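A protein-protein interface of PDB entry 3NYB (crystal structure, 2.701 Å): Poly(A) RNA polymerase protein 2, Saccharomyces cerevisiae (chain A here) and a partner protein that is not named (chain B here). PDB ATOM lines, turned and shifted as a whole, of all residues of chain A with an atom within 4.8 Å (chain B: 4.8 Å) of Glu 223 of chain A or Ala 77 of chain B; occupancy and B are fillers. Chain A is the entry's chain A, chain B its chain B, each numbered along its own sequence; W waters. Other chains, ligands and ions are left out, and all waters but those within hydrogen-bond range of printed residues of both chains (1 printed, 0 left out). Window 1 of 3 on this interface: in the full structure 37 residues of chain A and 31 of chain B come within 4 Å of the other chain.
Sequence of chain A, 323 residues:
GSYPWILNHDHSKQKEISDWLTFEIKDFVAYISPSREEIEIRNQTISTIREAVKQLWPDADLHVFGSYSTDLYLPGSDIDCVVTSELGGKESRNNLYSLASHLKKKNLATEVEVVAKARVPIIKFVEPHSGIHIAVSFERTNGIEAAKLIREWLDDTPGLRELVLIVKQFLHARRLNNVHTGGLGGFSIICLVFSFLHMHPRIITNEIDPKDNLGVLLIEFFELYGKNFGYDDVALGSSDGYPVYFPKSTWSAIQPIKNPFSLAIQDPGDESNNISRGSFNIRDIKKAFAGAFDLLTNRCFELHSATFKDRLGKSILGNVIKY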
ATOM      1  N   HIS A 200     -19.799 -13.861 -17.151  1.00  0.00           N
ATOM      2  CA  HIS A 200     -21.213 -13.555 -17.260  1.00  0.00           C
ATOM      3  C   HIS A 200     -21.969 -14.876 -17.282  1.00  0.00           C
ATOM      4  O   HIS A 200     -21.638 -15.763 -18.069  1.00  0.00           O
ATOM      5  CB  HIS A 200     -21.458 -12.761 -18.540  1.00  0.00           C
ATOM      6  CG  HIS A 200     -22.896 -12.458 -18.810  1.00  0.00           C
ATOM      7  ND1 HIS A 200     -23.811 -13.426 -19.166  1.00  0.00           N
ATOM      8  CD2 HIS A 200     -23.573 -11.284 -18.814  1.00  0.00           C
ATOM      9  CE1 HIS A 200     -24.992 -12.866 -19.359  1.00  0.00           C
ATOM     10  NE2 HIS A 200     -24.873 -11.565 -19.154  1.00  0.00           N
ATOM     11  N   PRO A 201     -22.980 -15.012 -16.410  1.00  0.00           N
ATOM     12  CA  PRO A 201     -23.752 -16.245 -16.191  1.00  0.00           C
ATOM     13  C   PRO A 201     -24.048 -17.026 -17.477  1.00  0.00           C
ATOM     14  O   PRO A 201     -23.895 -18.247 -17.509  1.00  0.00           O
ATOM     15  CB  PRO A 201     -25.049 -15.727 -15.573  1.00  0.00           C
ATOM     16  CG  PRO A 201     -24.632 -14.501 -14.832  1.00  0.00           C
ATOM     17  CD  PRO A 201     -23.497 -13.888 -15.608  1.00  0.00           C
ATOM     18  N   ILE A 219     -25.353  -3.160 -22.819  1.00  0.00           N
ATOM     19  CA  ILE A 219     -26.157  -2.623 -21.740  1.00  0.00           C
ATOM     20  C   ILE A 219     -25.692  -3.170 -20.396  1.00  0.00           C
ATOM     21  O   ILE A 219     -25.382  -2.409 -19.490  1.00  0.00           O
ATOM     22  CB  ILE A 219     -27.640  -2.917 -21.957  1.00  0.00           C
ATOM     23  CG1 ILE A 219     -28.172  -2.051 -23.096  1.00  0.00           C
ATOM     24  CG2 ILE A 219     -28.415  -2.651 -20.690  1.00  0.00           C
ATOM     25  CD1 ILE A 219     -29.620  -2.259 -23.378  1.00  0.00           C
ATOM     26  N   GLU A 220     -25.612  -4.490 -20.284  1.00  0.00           N
ATOM     27  CA  GLU A 220     -25.217  -5.119 -19.029  1.00  0.00           C
ATOM     28  C   GLU A 220     -23.804  -4.734 -18.580  1.00  0.00           C
ATOM     29  O   GLU A 220     -23.502  -4.737 -17.388  1.00  0.00           O
ATOM     30  CB  GLU A 220     -25.372  -6.639 -19.115  1.00  0.00           C
ATOM     31  CG  GLU A 220     -26.800  -7.076 -19.393  1.00  0.00           C
ATOM     32  CD  GLU A 220     -26.925  -8.559 -19.684  1.00  0.00           C
ATOM     33  OE1 GLU A 220     -25.889  -9.240 -19.823  1.00  0.00           O
ATOM     34  OE2 GLU A 220     -28.070  -9.042 -19.777  1.00  0.00           O
ATOM     35  N   PHE A 221     -22.937  -4.396 -19.524  1.00  0.00           N
ATOM     36  CA  PHE A 221     -21.618  -3.915 -19.152  1.00  0.00           C
ATOM     37  C   PHE A 221     -21.734  -2.591 -18.397  1.00  0.00           C
ATOM     38  O   PHE A 221     -21.087  -2.394 -17.374  1.00  0.00           O
ATOM     39  CB  PHE A 221     -20.721  -3.751 -20.383  1.00  0.00           C
ATOM     40  CG  PHE A 221     -19.464  -2.961 -20.117  1.00  0.00           C
ATOM     41  CD1 PHE A 221     -18.281  -3.598 -19.809  1.00  0.00           C
ATOM     42  CD2 PHE A 221     -19.468  -1.578 -20.184  1.00  0.00           C
ATOM     43  CE1 PHE A 221     -17.119  -2.875 -19.569  1.00  0.00           C
ATOM     44  CE2 PHE A 221     -18.313  -0.853 -19.946  1.00  0.00           C
ATOM     45  CZ  PHE A 221     -17.139  -1.502 -19.638  1.00  0.00           C
ATOM     46  N   PHE A 222     -22.547  -1.678 -18.910  1.00  0.00           N
ATOM     47  CA  PHE A 222     -22.729  -0.390 -18.250  1.00  0.00           C
ATOM     48  C   PHE A 222     -23.487  -0.544 -16.942  1.00  0.00           C
ATOM     49  O   PHE A 222     -23.351   0.268 -16.027  1.00  0.00           O
ATOM     50  CB  PHE A 222     -23.462   0.593 -19.164  1.00  0.00           C
ATOM     51  CG  PHE A 222     -22.646   1.050 -20.338  1.00  0.00           C
ATOM     52  CD1 PHE A 222     -21.387   1.594 -20.150  1.00  0.00           C
ATOM     53  CD2 PHE A 222     -23.142   0.943 -21.624  1.00  0.00           C
ATOM     54  CE1 PHE A 222     -20.636   2.014 -21.222  1.00  0.00           C
ATOM     55  CE2 PHE A 222     -22.398   1.358 -22.695  1.00  0.00           C
ATOM     56  CZ  PHE A 222     -21.141   1.897 -22.498  1.00  0.00           C
ATOM     57  N   GLU A 223     -24.294  -1.595 -16.865  1.00  0.00           N
ATOM     58  CA  GLU A 223     -25.074  -1.885 -15.675  1.00  0.00           C
ATOM     59  C   GLU A 223     -24.166  -2.388 -14.567  1.00  0.00           C
ATOM     60  O   GLU A 223     -24.256  -1.955 -13.421  1.00  0.00           O
ATOM     61  CB  GLU A 223     -26.124  -2.942 -15.997  1.00  0.00           C
ATOM     62  CG  GLU A 223     -26.918  -3.408 -14.806  1.00  0.00           C
ATOM     63  CD  GLU A 223     -27.851  -4.538 -15.154  1.00  0.00           C
ATOM     64  OE1 GLU A 223     -29.070  -4.399 -14.908  1.00  0.00           O
ATOM     65  OE2 GLU A 223     -27.357  -5.561 -15.682  1.00  0.00           O
ATOM     66  N   LEU A 224     -23.282  -3.309 -14.919  1.00  0.00           N
ATOM     67  CA  LEU A 224     -22.347  -3.849 -13.954  1.00  0.00           C
ATOM     68  C   LEU A 224     -21.477  -2.740 -13.399  1.00  0.00           C
ATOM     69  O   LEU A 224     -21.468  -2.487 -12.197  1.00  0.00           O
ATOM     70  CB  LEU A 224     -21.488  -4.940 -14.592  1.00  0.00           C
ATOM     71  CG  LEU A 224     -20.586  -5.707 -13.631  1.00  0.00           C
ATOM     72  CD1 LEU A 224     -19.301  -4.968 -13.402  1.00  0.00           C
ATOM     73  CD2 LEU A 224     -21.295  -5.945 -12.308  1.00  0.00           C
ATOM     74  N   TYR A 225     -20.758  -2.066 -14.288  1.00  0.00           N
ATOM     75  CA  TYR A 225     -19.747  -1.094 -13.887  1.00  0.00           C
ATOM     76  C   TYR A 225     -20.315   0.287 -13.606  1.00  0.00           C
ATOM     77  O   TYR A 225     -19.592   1.190 -13.199  1.00  0.00           O
ATOM     78  CB  TYR A 225     -18.648  -1.001 -14.943  1.00  0.00           C
ATOM     79  CG  TYR A 225     -17.860  -2.276 -15.104  1.00  0.00           C
ATOM     80  CD1 TYR A 225     -17.126  -2.795 -14.051  1.00  0.00           C
ATOM     81  CD2 TYR A 225     -17.841  -2.961 -16.310  1.00  0.00           C
ATOM     82  CE1 TYR A 225     -16.394  -3.958 -14.192  1.00  0.00           C
ATOM     83  CE2 TYR A 225     -17.114  -4.128 -16.457  1.00  0.00           C
ATOM     84  CZ  TYR A 225     -16.393  -4.619 -15.392  1.00  0.00           C
ATOM     85  OH  TYR A 225     -15.670  -5.779 -15.526  1.00  0.00           O
ATOM     86  N   GLY A 226     -21.613   0.453 -13.815  1.00  0.00           N
ATOM     87  CA  GLY A 226     -22.241   1.734 -13.552  1.00  0.00           C
ATOM     88  C   GLY A 226     -23.087   1.747 -12.288  1.00  0.00           C
ATOM     89  O   GLY A 226     -23.250   2.792 -11.659  1.00  0.00           O
ATOM     90  N   LYS A 227     -23.616   0.588 -11.903  1.00  0.00           N
ATOM     91  CA  LYS A 227     -24.613   0.531 -10.836  1.00  0.00           C
ATOM     92  C   LYS A 227     -24.292  -0.415  -9.685  1.00  0.00           C
ATOM     93  O   LYS A 227     -24.762  -0.203  -8.573  1.00  0.00           O
ATOM     94  CB  LYS A 227     -25.981   0.174 -11.415  1.00  0.00           C
ATOM     95  CG  LYS A 227     -26.583   1.280 -12.283  1.00  0.00           C
ATOM     96  CD  LYS A 227     -27.736   0.774 -13.141  1.00  0.00           C
ATOM     97  CE  LYS A 227     -28.948   0.364 -12.310  1.00  0.00           C
ATOM     98  NZ  LYS A 227     -29.932  -0.430 -13.114  1.00  0.00           N
ATOM     99  N   ASN A 228     -23.493  -1.446  -9.940  1.00  0.00           N
ATOM    100  CA  ASN A 228     -23.351  -2.529  -8.972  1.00  0.00           C
ATOM    101  C   ASN A 228     -21.946  -2.825  -8.485  1.00  0.00           C
ATOM    102  O   ASN A 228     -21.776  -3.336  -7.382  1.00  0.00           O
ATOM    103  CB  ASN A 228     -23.942  -3.816  -9.535  1.00  0.00           C
ATOM    104  CG  ASN A 228     -25.324  -3.615 -10.088  1.00  0.00           C
ATOM    105  OD1 ASN A 228     -26.176  -2.995  -9.453  1.00  0.00           O
ATOM    106  ND2 ASN A 228     -25.557  -4.132 -11.284  1.00  0.00           N
ATOM    107  N   PHE A 293     -26.111   3.383 -19.470  1.00  0.00           N
ATOM    108  CA  PHE A 293     -27.182   2.440 -19.189  1.00  0.00           C
ATOM    109  C   PHE A 293     -28.556   3.117 -19.270  1.00  0.00           C
ATOM    110  O   PHE A 293     -29.444   2.643 -19.974  1.00  0.00           O
ATOM    111  CB  PHE A 293     -26.970   1.837 -17.807  1.00  0.00           C
ATOM    112  CG  PHE A 293     -28.068   0.938 -17.374  1.00  0.00           C
ATOM    113  CD1 PHE A 293     -27.955  -0.431 -17.531  1.00  0.00           C
ATOM    114  CD2 PHE A 293     -29.218   1.454 -16.806  1.00  0.00           C
ATOM    115  CE1 PHE A 293     -28.968  -1.272 -17.131  1.00  0.00           C
ATOM    116  CE2 PHE A 293     -30.237   0.622 -16.407  1.00  0.00           C
ATOM    117  CZ  PHE A 293     -30.113  -0.745 -16.567  1.00  0.00           C
ATOM    118  N   TRP B  25     -35.375  -5.237 -23.098  1.00  0.00           N
ATOM    119  CA  TRP B  25     -34.026  -5.131 -23.629  1.00  0.00           C
ATOM    120  C   TRP B  25     -33.137  -6.294 -23.202  1.00  0.00           C
ATOM    121  O   TRP B  25     -32.148  -6.585 -23.860  1.00  0.00           O
ATOM    122  CB  TRP B  25     -33.394  -3.782 -23.259  1.00  0.00           C
ATOM    123  CG  TRP B  25     -33.229  -3.539 -21.783  1.00  0.00           C
ATOM    124  CD1 TRP B  25     -33.983  -2.713 -20.996  1.00  0.00           C
ATOM    125  CD2 TRP B  25     -32.241  -4.109 -20.925  1.00  0.00           C
ATOM    126  NE1 TRP B  25     -33.527  -2.740 -19.701  1.00  0.00           N
ATOM    127  CE2 TRP B  25     -32.446  -3.600 -19.632  1.00  0.00           C
ATOM    128  CE3 TRP B  25     -31.187  -5.013 -21.122  1.00  0.00           C
ATOM    129  CZ2 TRP B  25     -31.658  -3.945 -18.547  1.00  0.00           C
ATOM    130  CZ3 TRP B  25     -30.401  -5.366 -20.042  1.00  0.00           C
ATOM    131  CH2 TRP B  25     -30.638  -4.834 -18.773  1.00  0.00           C
ATOM    132  N   ARG B  26     -33.488  -6.959 -22.107  1.00  0.00           N
ATOM    133  CA  ARG B  26     -32.688  -8.084 -21.640  1.00  0.00           C
ATOM    134  C   ARG B  26     -33.184  -9.388 -22.248  1.00  0.00           C
ATOM    135  O   ARG B  26     -33.910 -10.156 -21.606  1.00  0.00           O
ATOM    136  CB  ARG B  26     -32.681  -8.167 -20.119  1.00  0.00           C
ATOM    137  CG  ARG B  26     -31.793  -9.271 -19.574  1.00  0.00           C
ATOM    138  CD  ARG B  26     -31.606  -9.120 -18.079  1.00  0.00           C
ATOM    139  NE  ARG B  26     -30.519  -8.200 -17.769  1.00  0.00           N
ATOM    140  CZ  ARG B  26     -30.509  -7.371 -16.729  1.00  0.00           C
ATOM    141  NH1 ARG B  26     -31.539  -7.318 -15.893  1.00  0.00           N
ATOM    142  NH2 ARG B  26     -29.470  -6.578 -16.534  1.00  0.00           N
ATOM    143  N   TYR B  28     -31.690 -12.803 -24.580  1.00  0.00           N
ATOM    144  CA  TYR B  28     -30.513 -13.504 -25.076  1.00  0.00           C
ATOM    145  C   TYR B  28     -30.874 -14.417 -26.236  1.00  0.00           C
ATOM    146  O   TYR B  28     -31.894 -15.103 -26.209  1.00  0.00           O
ATOM    147  CB  TYR B  28     -29.866 -14.341 -23.972  1.00  0.00           C
ATOM    148  CG  TYR B  28     -29.543 -13.567 -22.720  1.00  0.00           C
ATOM    149  CD1 TYR B  28     -28.565 -12.585 -22.721  1.00  0.00           C
ATOM    150  CD2 TYR B  28     -30.210 -13.826 -21.533  1.00  0.00           C
ATOM    151  CE1 TYR B  28     -28.260 -11.877 -21.574  1.00  0.00           C
ATOM    152  CE2 TYR B  28     -29.915 -13.122 -20.382  1.00  0.00           C
ATOM    153  CZ  TYR B  28     -28.940 -12.149 -20.407  1.00  0.00           C
ATOM    154  OH  TYR B  28     -28.647 -11.441 -19.264  1.00  0.00           O
ATOM    155  N   GLY B  75     -33.266  -6.814 -10.276  1.00  0.00           N
ATOM    156  CA  GLY B  75     -31.968  -7.466 -10.367  1.00  0.00           C
ATOM    157  C   GLY B  75     -31.023  -7.064 -11.491  1.00  0.00           C
ATOM    158  O   GLY B  75     -31.363  -6.275 -12.377  1.00  0.00           O
ATOM    159  N   SER B  76     -29.815  -7.618 -11.448  1.00  0.00           N
ATOM    160  CA  SER B  76     -28.852  -7.428 -12.525  1.00  0.00           C
ATOM    161  C   SER B  76     -28.707  -8.668 -13.371  1.00  0.00           C
ATOM    162  O   SER B  76     -29.418  -9.654 -13.200  1.00  0.00           O
ATOM    163  CB  SER B  76     -27.477  -7.071 -11.978  1.00  0.00           C
ATOM    164  OG  SER B  76     -27.368  -5.679 -11.782  1.00  0.00           O
ATOM    165  N   ALA B  77     -27.759  -8.603 -14.289  1.00  0.00           N
ATOM    166  CA  ALA B  77     -27.386  -9.746 -15.088  1.00  0.00           C
ATOM    167  C   ALA B  77     -26.765 -10.783 -14.170  1.00  0.00           C
ATOM    168  O   ALA B  77     -26.857 -11.985 -14.414  1.00  0.00           O
ATOM    169  CB  ALA B  77     -26.396  -9.323 -16.147  1.00  0.00           C
ATOM    170  N   PHE B  78     -26.142 -10.305 -13.100  1.00  0.00           N
ATOM    171  CA  PHE B  78     -25.306 -11.159 -12.274  1.00  0.00           C
ATOM    172  C   PHE B  78     -25.993 -11.735 -11.035  1.00  0.00           C
ATOM    173  O   PHE B  78     -25.522 -11.556  -9.915  1.00  0.00           O
ATOM    174  CB  PHE B  78     -24.016 -10.427 -11.903  1.00  0.00           C
ATOM    175  CG  PHE B  78     -23.082 -10.254 -13.057  1.00  0.00           C
ATOM    176  CD1 PHE B  78     -22.114 -11.204 -13.327  1.00  0.00           C
ATOM    177  CD2 PHE B  78     -23.188  -9.154 -13.892  1.00  0.00           C
ATOM    178  CE1 PHE B  78     -21.256 -11.055 -14.397  1.00  0.00           C
ATOM    179  CE2 PHE B  78     -22.334  -8.995 -14.963  1.00  0.00           C
ATOM    180  CZ  PHE B  78     -21.364  -9.949 -15.217  1.00  0.00           C
ATOM    181  N   THR B  79     -27.100 -12.438 -11.249  1.00  0.00           N
ATOM    182  CA  THR B  79     -27.748 -13.200 -10.194  1.00  0.00           C
ATOM    183  C   THR B  79     -27.607 -14.671 -10.534  1.00  0.00           C
ATOM    184  O   THR B  79     -27.394 -15.018 -11.689  1.00  0.00           O
ATOM    185  CB  THR B  79     -29.243 -12.880 -10.097  1.00  0.00           C
ATOM    186  OG1 THR B  79     -29.893 -13.292 -11.304  1.00  0.00           O
ATOM    187  CG2 THR B  79     -29.467 -11.393  -9.894  1.00  0.00           C
ATOM    188  N   LEU B  83     -29.315 -15.562 -15.548  1.00  0.00           N
ATOM    189  CA  LEU B  83     -29.820 -14.747 -16.648  1.00  0.00           C
ATOM    190  C   LEU B  83     -28.933 -13.535 -16.897  1.00  0.00           C
ATOM    191  O   LEU B  83     -27.751 -13.540 -16.551  1.00  0.00           O
ATOM    192  CB  LEU B  83     -31.268 -14.318 -16.381  1.00  0.00           C
ATOM    193  CG  LEU B  83     -31.685 -14.088 -14.922  1.00  0.00           C
ATOM    194  CD1 LEU B  83     -31.121 -12.783 -14.378  1.00  0.00           C
ATOM    195  CD2 LEU B  83     -33.203 -14.112 -14.785  1.00  0.00           C
HETATM  196  O   HOH W   1     -24.643  -6.412 -12.393  1.00  0.00           O
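The side-chain carboxylate (OE2) of Glu 220 of chain A lies within salt-bridge range of the guanidinium group (NE) of Arg 26 of chain B, 3.3 Å away.
The side-chain carboxylate (OE2) of Glu 220 of chain A lies within hydrogen-bond range of the side-chain hydroxyl (OH) of Tyr 28 of chain B (2.5 Å).
NH2 of Arg 26 of chain B is in salt-bridge range of OE2 of Glu 223 of chain A (2.5 Å).
The side-chain carboxylate of Glu 223 of chain A is in hydrogen-bond range of the backbone NH of Ala 77 of chain B.
The side-chain amide nitrogen of Asn 228 of chain A is in hydrogen-bond range of the side-chain hydroxyl of Ser 76 of chain B (2.4 Å).
NE2 of His 200 of chain A lies within hydrogen-bond range of OE1 of Glu 220 of chain A (2.6 Å).
The backbone carbonyl oxygen (O) of Glu 223 of chain A lies within hydrogen-bond range of the side-chain amide nitrogen (ND2) of Asn 228 of chain A, 3.3 Å away.
NE2 of His 200 of chain A touches OH of Tyr 28 of chain B, at 3.8 Å.
CE1 of Phe 78 of chain B touches CA of His 200 of chain A, 3.8 Å away.
His 200 of chain A touches Leu 83 of chain B.
Pro 201 of chain A touches Ala 77 of chain B.
Pro 201 of chain A touches Phe 78 of chain B.
Ile 219 of chain A touches Trp 25 of chain B (CG2 to CZ3, 3.4 Å).
Ala 77 of chain B touches Glu 220 of chain A (CB to CD, 3.7 Å).
Glu 223 of chain A touches Gly 75 of chain B.
Glu 223 of chain A touches Ser 76 of chain B (CD to OG, 3.6 Å).
Phe 78 of chain B touches Leu 224 of chain A (CE2 to CG, 3.95 Å).
Glu 223 of chain A touches just these residues of chain B: Arg 26 (2.5 Å), Gly 75 (3.9 Å), Ser 76 (3.6 Å) and Ala 77 (3.4 Å).
Printed residues of chain B within 4 Å of Leu 224 of chain A: Phe 78.
Of the printed residues of chain A, Tyr 28 of chain B touches His 200 and Glu 220.
The nearest residue of chain A that does not touch Ala 77 of chain B is His 200 of chain A (4.05 Å).
Of the 9 printed residues of chain B, 8 touch a printed residue of chain A.
Hydrophobic or aromatic side chains of chain B that line the printed part of chain A: Trp 25, Tyr 28, Ala 77 and Phe 78.
Of the 13 printed residues of chain A, 7 touch a printed residue of chain B.
Among the printed residues, 16 pairs touch across the chains.
Water W1 bridges ND2 of Asn 228 of chain A (2.7 Å) and OG of Ser 76 of chain B (2.9 Å).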
